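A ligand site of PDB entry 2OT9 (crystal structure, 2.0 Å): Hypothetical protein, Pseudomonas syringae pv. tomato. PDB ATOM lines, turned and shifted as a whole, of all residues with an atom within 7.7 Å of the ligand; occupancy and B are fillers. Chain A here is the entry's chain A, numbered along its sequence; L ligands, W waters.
NE of Arg 39 sits close to OH of Tyr 107 (3.3 Å).
The side-chain carboxylate (OD1) of Asp 88 sits at hydrogen-bond distance from the backbone NH (N) of Arg 91 (2.9 Å).
The backbone carbonyl oxygen (O) of Val 84 sits at hydrogen-bond distance from the guanidinium group (NH1) of Arg 39.
The guanidinium group of Arg 91 is in hydrogen-bond range of the backbone carbonyl oxygen of Glu 66.
The backbone carbonyl oxygen (O) of Leu 105 lies within hydrogen-bond range of the backbone NH (N) of Gly 85 (3.0 Å).
The guanidinium group of Arg 91 lies within hydrogen-bond range of the backbone carbonyl oxygen of Val 64 (2.7 Å).
NE2 of Gln 86 sits at hydrogen-bond distance from O of Tyr 107 (3.0 Å).
NE1 of Trp 113 lies within hydrogen-bond range of O of Pro 87, at 2.9 Å.
Water W3 lies within hydrogen-bond range of the side-chain carboxylate of Glu 83 (2.6 Å), an oxygen (O4) of the ligand (2.9 Å) and the backbone NH of Val 84 (2.9 Å).
Water W4 bridges the guanidinium group of Arg 39 and an oxygen (O5) of the ligand.
Residues that only touch the ligand: Gly 85, Leu 61 and Pro 87.
Hydrophobic or aromatic side chains within 4 Å of the ligand: Leu 61 and Pro 87.
N of Gln 86 lies within hydrogen-bond range of O1 of the ligand.
An oxygen (O4) of the ligand sits at hydrogen-bond distance from the backbone carbonyl oxygen (O) of Val 84, 2.7 Å away.
The guanidinium group (NE) of Arg 91 lies within salt-bridge range of an oxygen (O6) of the ligand (3.5 Å).
NH2 of Arg 39 is in salt-bridge range of O1 of the ligand.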
ATOM      1  N   SER A  34     -19.001   8.118   7.784  1.00  0.00           N
ATOM      2  CA  SER A  34     -17.847   7.725   8.597  1.00  0.00           C
ATOM      3  C   SER A  34     -18.070   6.456   9.435  1.00  0.00           C
ATOM      4  O   SER A  34     -17.120   5.938  10.033  1.00  0.00           O
ATOM      5  CB  SER A  34     -17.453   8.861   9.540  1.00  0.00           C
ATOM      6  OG  SER A  34     -17.048   9.976   8.782  1.00  0.00           O
ATOM      7  N   ARG A  39     -18.854  -0.934  12.465  1.00  0.00           N
ATOM      8  CA  ARG A  39     -19.366  -0.085  13.549  1.00  0.00           C
ATOM      9  C   ARG A  39     -20.882  -0.191  13.660  1.00  0.00           C
ATOM     10  O   ARG A  39     -21.433  -0.407  14.741  1.00  0.00           O
ATOM     11  CB  ARG A  39     -18.941   1.376  13.336  1.00  0.00           C
ATOM     12  CG  ARG A  39     -19.431   2.315  14.464  1.00  0.00           C
ATOM     13  CD  ARG A  39     -18.834   3.730  14.325  1.00  0.00           C
ATOM     14  NE  ARG A  39     -17.400   3.700  14.606  1.00  0.00           N
ATOM     15  CZ  ARG A  39     -16.860   3.858  15.808  1.00  0.00           C
ATOM     16  NH1 ARG A  39     -17.627   4.107  16.866  1.00  0.00           N
ATOM     17  NH2 ARG A  39     -15.527   3.806  15.959  1.00  0.00           N
ATOM     18  N   ARG A  59     -27.283   9.526  17.447  1.00  0.00           N
ATOM     19  CA  ARG A  59     -26.531   9.959  16.259  1.00  0.00           C
ATOM     20  C   ARG A  59     -25.073   9.497  16.275  1.00  0.00           C
ATOM     21  O   ARG A  59     -24.299   9.846  15.372  1.00  0.00           O
ATOM     22  CB  ARG A  59     -26.655  11.463  16.034  1.00  0.00           C
ATOM     23  CG  ARG A  59     -28.092  11.946  15.754  1.00  0.00           C
ATOM     24  CD  ARG A  59     -28.129  13.391  15.280  1.00  0.00           C
ATOM     25  NE  ARG A  59     -27.935  13.521  13.831  1.00  0.00           N
ATOM     26  CZ  ARG A  59     -28.809  14.071  12.991  1.00  0.00           C
ATOM     27  NH1 ARG A  59     -29.956  14.572  13.428  1.00  0.00           N
ATOM     28  NH2 ARG A  59     -28.521  14.141  11.692  1.00  0.00           N
ATOM     29  N   GLY A  60     -24.691   8.728  17.311  1.00  0.00           N
ATOM     30  CA  GLY A  60     -23.376   8.069  17.398  1.00  0.00           C
ATOM     31  C   GLY A  60     -22.210   8.981  17.038  1.00  0.00           C
ATOM     32  O   GLY A  60     -22.164  10.139  17.487  1.00  0.00           O
ATOM     33  N   LEU A  61     -21.288   8.489  16.207  1.00  0.00           N
ATOM     34  CA  LEU A  61     -20.076   9.240  15.850  1.00  0.00           C
ATOM     35  C   LEU A  61     -20.302  10.590  15.169  1.00  0.00           C
ATOM     36  O   LEU A  61     -19.400  11.435  15.157  1.00  0.00           O
ATOM     37  CB  LEU A  61     -19.080   8.365  15.039  1.00  0.00           C
ATOM     38  CG  LEU A  61     -19.391   7.727  13.683  1.00  0.00           C
ATOM     39  CD1 LEU A  61     -20.087   8.667  12.718  1.00  0.00           C
ATOM     40  CD2 LEU A  61     -18.086   7.224  13.068  1.00  0.00           C
ATOM     41  N   SER A  62     -21.493  10.815  14.618  1.00  0.00           N
ATOM     42  CA  SER A  62     -21.787  12.080  13.913  1.00  0.00           C
ATOM     43  C   SER A  62     -22.146  13.264  14.828  1.00  0.00           C
ATOM     44  O   SER A  62     -22.219  14.414  14.366  1.00  0.00           O
ATOM     45  CB  SER A  62     -22.867  11.852  12.834  1.00  0.00           C
ATOM     46  OG  SER A  62     -24.177  12.046  13.341  1.00  0.00           O
ATOM     47  N   ASP A  63     -22.380  12.987  16.116  1.00  0.00           N
ATOM     48  CA  ASP A  63     -22.705  14.033  17.117  1.00  0.00           C
ATOM     49  C   ASP A  63     -22.046  13.702  18.456  1.00  0.00           C
ATOM     50  O   ASP A  63     -22.431  12.735  19.114  1.00  0.00           O
ATOM     51  CB  ASP A  63     -24.225  14.132  17.294  1.00  0.00           C
ATOM     52  CG  ASP A  63     -24.653  15.248  18.262  1.00  0.00           C
ATOM     53  OD1 ASP A  63     -23.829  15.783  19.037  1.00  0.00           O
ATOM     54  OD2 ASP A  63     -25.860  15.601  18.238  1.00  0.00           O
ATOM     55  N   VAL A  64     -21.079  14.521  18.867  1.00  0.00           N
ATOM     56  CA  VAL A  64     -20.340  14.268  20.098  1.00  0.00           C
ATOM     57  C   VAL A  64     -21.203  14.241  21.364  1.00  0.00           C
ATOM     58  O   VAL A  64     -20.844  13.613  22.354  1.00  0.00           O
ATOM     59  CB  VAL A  64     -19.148  15.245  20.286  1.00  0.00           C
ATOM     60  CG1 VAL A  64     -18.037  14.926  19.286  1.00  0.00           C
ATOM     61  CG2 VAL A  64     -19.610  16.697  20.196  1.00  0.00           C
ATOM     62  N   GLU A  66     -24.160  12.882  21.704  1.00  0.00           N
ATOM     63  CA  GLU A  66     -25.052  11.720  21.719  1.00  0.00           C
ATOM     64  C   GLU A  66     -24.263  10.396  21.729  1.00  0.00           C
ATOM     65  O   GLU A  66     -23.146  10.340  21.241  1.00  0.00           O
ATOM     66  CB  GLU A  66     -26.018  11.762  20.530  1.00  0.00           C
ATOM     67  CG  GLU A  66     -27.044  12.906  20.588  1.00  0.00           C
ATOM     68  CD  GLU A  66     -28.329  12.610  19.826  1.00  0.00           C
ATOM     69  OE1 GLU A  66     -28.523  11.474  19.340  1.00  0.00           O
ATOM     70  OE2 GLU A  66     -29.178  13.539  19.753  1.00  0.00           O
ATOM     71  N   PRO A  67     -24.832   9.341  22.329  1.00  0.00           N
ATOM     72  CA  PRO A  67     -24.203   8.020  22.275  1.00  0.00           C
ATOM     73  C   PRO A  67     -24.596   7.265  21.004  1.00  0.00           C
ATOM     74  O   PRO A  67     -25.439   7.743  20.239  1.00  0.00           O
ATOM     75  CB  PRO A  67     -24.787   7.305  23.478  1.00  0.00           C
ATOM     76  CG  PRO A  67     -26.166   7.917  23.633  1.00  0.00           C
ATOM     77  CD  PRO A  67     -26.077   9.327  23.122  1.00  0.00           C
ATOM     78  N   ALA A  68     -24.021   6.079  20.822  1.00  0.00           N
ATOM     79  CA  ALA A  68     -24.433   5.156  19.781  1.00  0.00           C
ATOM     80  C   ALA A  68     -25.861   4.673  20.027  1.00  0.00           C
ATOM     81  O   ALA A  68     -26.674   4.618  19.098  1.00  0.00           O
ATOM     82  CB  ALA A  68     -23.470   3.979  19.740  1.00  0.00           C
ATOM     83  N   ILE A  82     -25.054   3.858  25.846  1.00  0.00           N
ATOM     84  CA  ILE A  82     -24.248   2.831  25.200  1.00  0.00           C
ATOM     85  C   ILE A  82     -23.346   3.384  24.113  1.00  0.00           C
ATOM     86  O   ILE A  82     -23.813   4.001  23.148  1.00  0.00           O
ATOM     87  CB  ILE A  82     -25.136   1.723  24.578  1.00  0.00           C
ATOM     88  CG1 ILE A  82     -26.177   1.260  25.607  1.00  0.00           C
ATOM     89  CG2 ILE A  82     -24.279   0.550  24.079  1.00  0.00           C
ATOM     90  CD1 ILE A  82     -27.164   0.175  25.129  1.00  0.00           C
ATOM     91  N   GLU A  83     -22.042   3.150  24.245  1.00  0.00           N
ATOM     92  CA  GLU A  83     -21.121   3.497  23.161  1.00  0.00           C
ATOM     93  C   GLU A  83     -20.603   2.250  22.469  1.00  0.00           C
ATOM     94  O   GLU A  83     -20.722   1.131  22.990  1.00  0.00           O
ATOM     95  CB  GLU A  83     -19.926   4.297  23.708  1.00  0.00           C
ATOM     96  CG  GLU A  83     -20.303   5.645  24.332  1.00  0.00           C
ATOM     97  CD  GLU A  83     -20.769   6.711  23.309  1.00  0.00           C
ATOM     98  OE1 GLU A  83     -21.047   6.401  22.108  1.00  0.00           O
ATOM     99  OE2 GLU A  83     -20.890   7.866  23.720  1.00  0.00           O
ATOM    100  N   VAL A  84     -20.015   2.443  21.290  1.00  0.00           N
ATOM    101  CA  VAL A  84     -19.343   1.365  20.575  1.00  0.00           C
ATOM    102  C   VAL A  84     -17.959   1.866  20.123  1.00  0.00           C
ATOM    103  O   VAL A  84     -17.771   3.061  19.927  1.00  0.00           O
ATOM    104  CB  VAL A  84     -20.162   0.795  19.367  1.00  0.00           C
ATOM    105  CG1 VAL A  84     -21.583   0.369  19.817  1.00  0.00           C
ATOM    106  CG2 VAL A  84     -20.243   1.793  18.235  1.00  0.00           C
ATOM    107  N   GLY A  85     -17.016   0.955  19.971  1.00  0.00           N
ATOM    108  CA  GLY A  85     -15.688   1.320  19.460  1.00  0.00           C
ATOM    109  C   GLY A  85     -14.691   1.567  20.576  1.00  0.00           C
ATOM    110  O   GLY A  85     -14.634   0.800  21.546  1.00  0.00           O
ATOM    111  N   GLN A  86     -13.934   2.660  20.466  1.00  0.00           N
ATOM    112  CA  GLN A  86     -12.827   2.917  21.380  1.00  0.00           C
ATOM    113  C   GLN A  86     -12.864   4.350  21.934  1.00  0.00           C
ATOM    114  O   GLN A  86     -11.933   5.124  21.702  1.00  0.00           O
ATOM    115  CB  GLN A  86     -11.489   2.635  20.665  1.00  0.00           C
ATOM    116  CG  GLN A  86     -11.314   1.158  20.289  1.00  0.00           C
ATOM    117  CD  GLN A  86     -10.007   0.841  19.590  1.00  0.00           C
ATOM    118  OE1 GLN A  86      -9.038   1.601  19.674  1.00  0.00           O
ATOM    119  NE2 GLN A  86      -9.984  -0.283  18.883  1.00  0.00           N
ATOM    120  N   PRO A  87     -13.940   4.712  22.685  1.00  0.00           N
ATOM    121  CA  PRO A  87     -13.959   6.054  23.285  1.00  0.00           C
ATOM    122  C   PRO A  87     -12.876   6.145  24.363  1.00  0.00           C
ATOM    123  O   PRO A  87     -12.490   5.122  24.933  1.00  0.00           O
ATOM    124  CB  PRO A  87     -15.346   6.128  23.944  1.00  0.00           C
ATOM    125  CG  PRO A  87     -15.730   4.697  24.186  1.00  0.00           C
ATOM    126  CD  PRO A  87     -15.137   3.911  23.043  1.00  0.00           C
ATOM    127  N   ASP A  88     -12.351   7.347  24.611  1.00  0.00           N
ATOM    128  CA  ASP A  88     -11.313   7.505  25.638  1.00  0.00           C
ATOM    129  C   ASP A  88     -11.903   7.578  27.058  1.00  0.00           C
ATOM    130  O   ASP A  88     -13.119   7.671  27.220  1.00  0.00           O
ATOM    131  CB  ASP A  88     -10.334   8.661  25.310  1.00  0.00           C
ATOM    132  CG  ASP A  88     -10.979  10.061  25.354  1.00  0.00           C
ATOM    133  OD1 ASP A  88     -11.966  10.285  26.093  1.00  0.00           O
ATOM    134  OD2 ASP A  88     -10.461  10.967  24.641  1.00  0.00           O
ATOM    135  N   ARG A  91     -14.174  10.638  27.935  1.00  0.00           N
ATOM    136  CA  ARG A  91     -15.546  10.570  27.401  1.00  0.00           C
ATOM    137  C   ARG A  91     -16.406   9.639  28.253  1.00  0.00           C
ATOM    138  O   ARG A  91     -17.541   9.987  28.613  1.00  0.00           O
ATOM    139  CB  ARG A  91     -15.569  10.104  25.934  1.00  0.00           C
ATOM    140  CG  ARG A  91     -17.008  10.045  25.372  1.00  0.00           C
ATOM    141  CD  ARG A  91     -17.130   9.852  23.867  1.00  0.00           C
ATOM    142  NE  ARG A  91     -18.548   9.731  23.496  1.00  0.00           N
ATOM    143  CZ  ARG A  91     -19.374  10.754  23.247  1.00  0.00           C
ATOM    144  NH1 ARG A  91     -18.932  12.011  23.302  1.00  0.00           N
ATOM    145  NH2 ARG A  91     -20.646  10.509  22.923  1.00  0.00           N
ATOM    146  N   CYS A  95     -19.672  11.055  30.190  1.00  0.00           N
ATOM    147  CA  CYS A  95     -20.937  10.443  29.816  1.00  0.00           C
ATOM    148  C   CYS A  95     -21.551   9.685  30.991  1.00  0.00           C
ATOM    149  O   CYS A  95     -22.747   9.804  31.229  1.00  0.00           O
ATOM    150  CB  CYS A  95     -20.798   9.552  28.582  1.00  0.00           C
ATOM    151  SG  CYS A  95     -20.399  10.500  27.062  1.00  0.00           S
ATOM    152  N   LEU A 104     -20.209  -0.136  27.093  1.00  0.00           N
ATOM    153  CA  LEU A 104     -19.439   0.010  25.864  1.00  0.00           C
ATOM    154  C   LEU A 104     -19.248  -1.357  25.247  1.00  0.00           C
ATOM    155  O   LEU A 104     -18.761  -2.280  25.917  1.00  0.00           O
ATOM    156  CB  LEU A 104     -18.083   0.662  26.148  1.00  0.00           C
ATOM    157  CG  LEU A 104     -17.030   0.568  25.042  1.00  0.00           C
ATOM    158  CD1 LEU A 104     -17.461   1.359  23.772  1.00  0.00           C
ATOM    159  CD2 LEU A 104     -15.684   1.054  25.559  1.00  0.00           C
ATOM    160  N   LEU A 105     -19.616  -1.486  23.963  1.00  0.00           N
ATOM    161  CA  LEU A 105     -19.186  -2.620  23.161  1.00  0.00           C
ATOM    162  C   LEU A 105     -17.982  -2.210  22.336  1.00  0.00           C
ATOM    163  O   LEU A 105     -18.133  -1.544  21.282  1.00  0.00           O
ATOM    164  CB  LEU A 105     -20.292  -3.140  22.222  1.00  0.00           C
ATOM    165  CG  LEU A 105     -21.396  -4.015  22.779  1.00  0.00           C
ATOM    166  CD1 LEU A 105     -22.206  -4.615  21.634  1.00  0.00           C
ATOM    167  CD2 LEU A 105     -20.786  -5.141  23.661  1.00  0.00           C
ATOM    168  N   ALA A 106     -16.802  -2.603  22.788  1.00  0.00           N
ATOM    169  CA  ALA A 106     -15.561  -2.217  22.158  1.00  0.00           C
ATOM    170  C   ALA A 106     -15.270  -3.172  21.004  1.00  0.00           C
ATOM    171  O   ALA A 106     -15.728  -4.310  21.011  1.00  0.00           O
ATOM    172  CB  ALA A 106     -14.435  -2.252  23.200  1.00  0.00           C
ATOM    173  N   TYR A 107     -14.560  -2.697  19.977  1.00  0.00           N
ATOM    174  CA  TYR A 107     -14.118  -3.577  18.893  1.00  0.00           C
ATOM    175  C   TYR A 107     -12.847  -3.018  18.287  1.00  0.00           C
ATOM    176  O   TYR A 107     -12.445  -1.893  18.604  1.00  0.00           O
ATOM    177  CB  TYR A 107     -15.225  -3.789  17.833  1.00  0.00           C
ATOM    178  CG  TYR A 107     -15.457  -2.589  16.939  1.00  0.00           C
ATOM    179  CD1 TYR A 107     -14.817  -2.498  15.671  1.00  0.00           C
ATOM    180  CD2 TYR A 107     -16.303  -1.557  17.326  1.00  0.00           C
ATOM    181  CE1 TYR A 107     -15.015  -1.397  14.848  1.00  0.00           C
ATOM    182  CE2 TYR A 107     -16.505  -0.428  16.507  1.00  0.00           C
ATOM    183  CZ  TYR A 107     -15.860  -0.363  15.273  1.00  0.00           C
ATOM    184  OH  TYR A 107     -16.030   0.732  14.462  1.00  0.00           O
ATOM    185  N   TRP A 113      -5.397   0.587  23.569  1.00  0.00           N
ATOM    186  CA  TRP A 113      -6.590   1.205  24.186  1.00  0.00           C
ATOM    187  C   TRP A 113      -6.860   0.728  25.621  1.00  0.00           C
ATOM    188  O   TRP A 113      -7.017   1.542  26.536  1.00  0.00           O
ATOM    189  CB  TRP A 113      -7.815   0.937  23.295  1.00  0.00           C
ATOM    190  CG  TRP A 113      -9.084   1.500  23.826  1.00  0.00           C
ATOM    191  CD1 TRP A 113      -9.563   2.765  23.624  1.00  0.00           C
ATOM    192  CD2 TRP A 113     -10.038   0.834  24.661  1.00  0.00           C
ATOM    193  NE1 TRP A 113     -10.768   2.924  24.266  1.00  0.00           N
ATOM    194  CE2 TRP A 113     -11.072   1.758  24.927  1.00  0.00           C
ATOM    195  CE3 TRP A 113     -10.111  -0.444  25.222  1.00  0.00           C
ATOM    196  CZ2 TRP A 113     -12.174   1.439  25.718  1.00  0.00           C
ATOM    197  CZ3 TRP A 113     -11.210  -0.777  26.011  1.00  0.00           C
ATOM    198  CH2 TRP A 113     -12.227   0.169  26.241  1.00  0.00           C
HETATM  199  O1  LIG L   1     -14.671   4.420  18.574  1.00  0.00           O
HETATM  200  O2  LIG L   1     -13.709   6.369  18.762  1.00  0.00           O
HETATM  201  C1  LIG L   1     -14.716   5.650  18.559  1.00  0.00           C
HETATM  202  C2  LIG L   1     -16.070   6.270  18.309  1.00  0.00           C
HETATM  203  O3  LIG L   1     -16.124   7.263  17.277  1.00  0.00           O
HETATM  204  C3  LIG L   1     -16.547   6.806  19.631  1.00  0.00           C
HETATM  205  O4  LIG L   1     -17.051   5.648  20.301  1.00  0.00           O
HETATM  206  C4  LIG L   1     -17.590   7.893  19.484  1.00  0.00           C
HETATM  207  O5  LIG L   1     -18.522   7.794  18.638  1.00  0.00           O
HETATM  208  O6  LIG L   1     -17.485   8.884  20.225  1.00  0.00           O
HETATM  209  O   HOH W   1     -19.098  10.835  19.437  1.00  0.00           O
HETATM  210  O   HOH W   2     -21.059   8.174  19.822  1.00  0.00           O
HETATM  211  O   HOH W   3     -19.938   5.155  20.173  1.00  0.00           O
HETATM  212  O   HOH W   4     -20.259   5.252  17.197  1.00  0.00           O
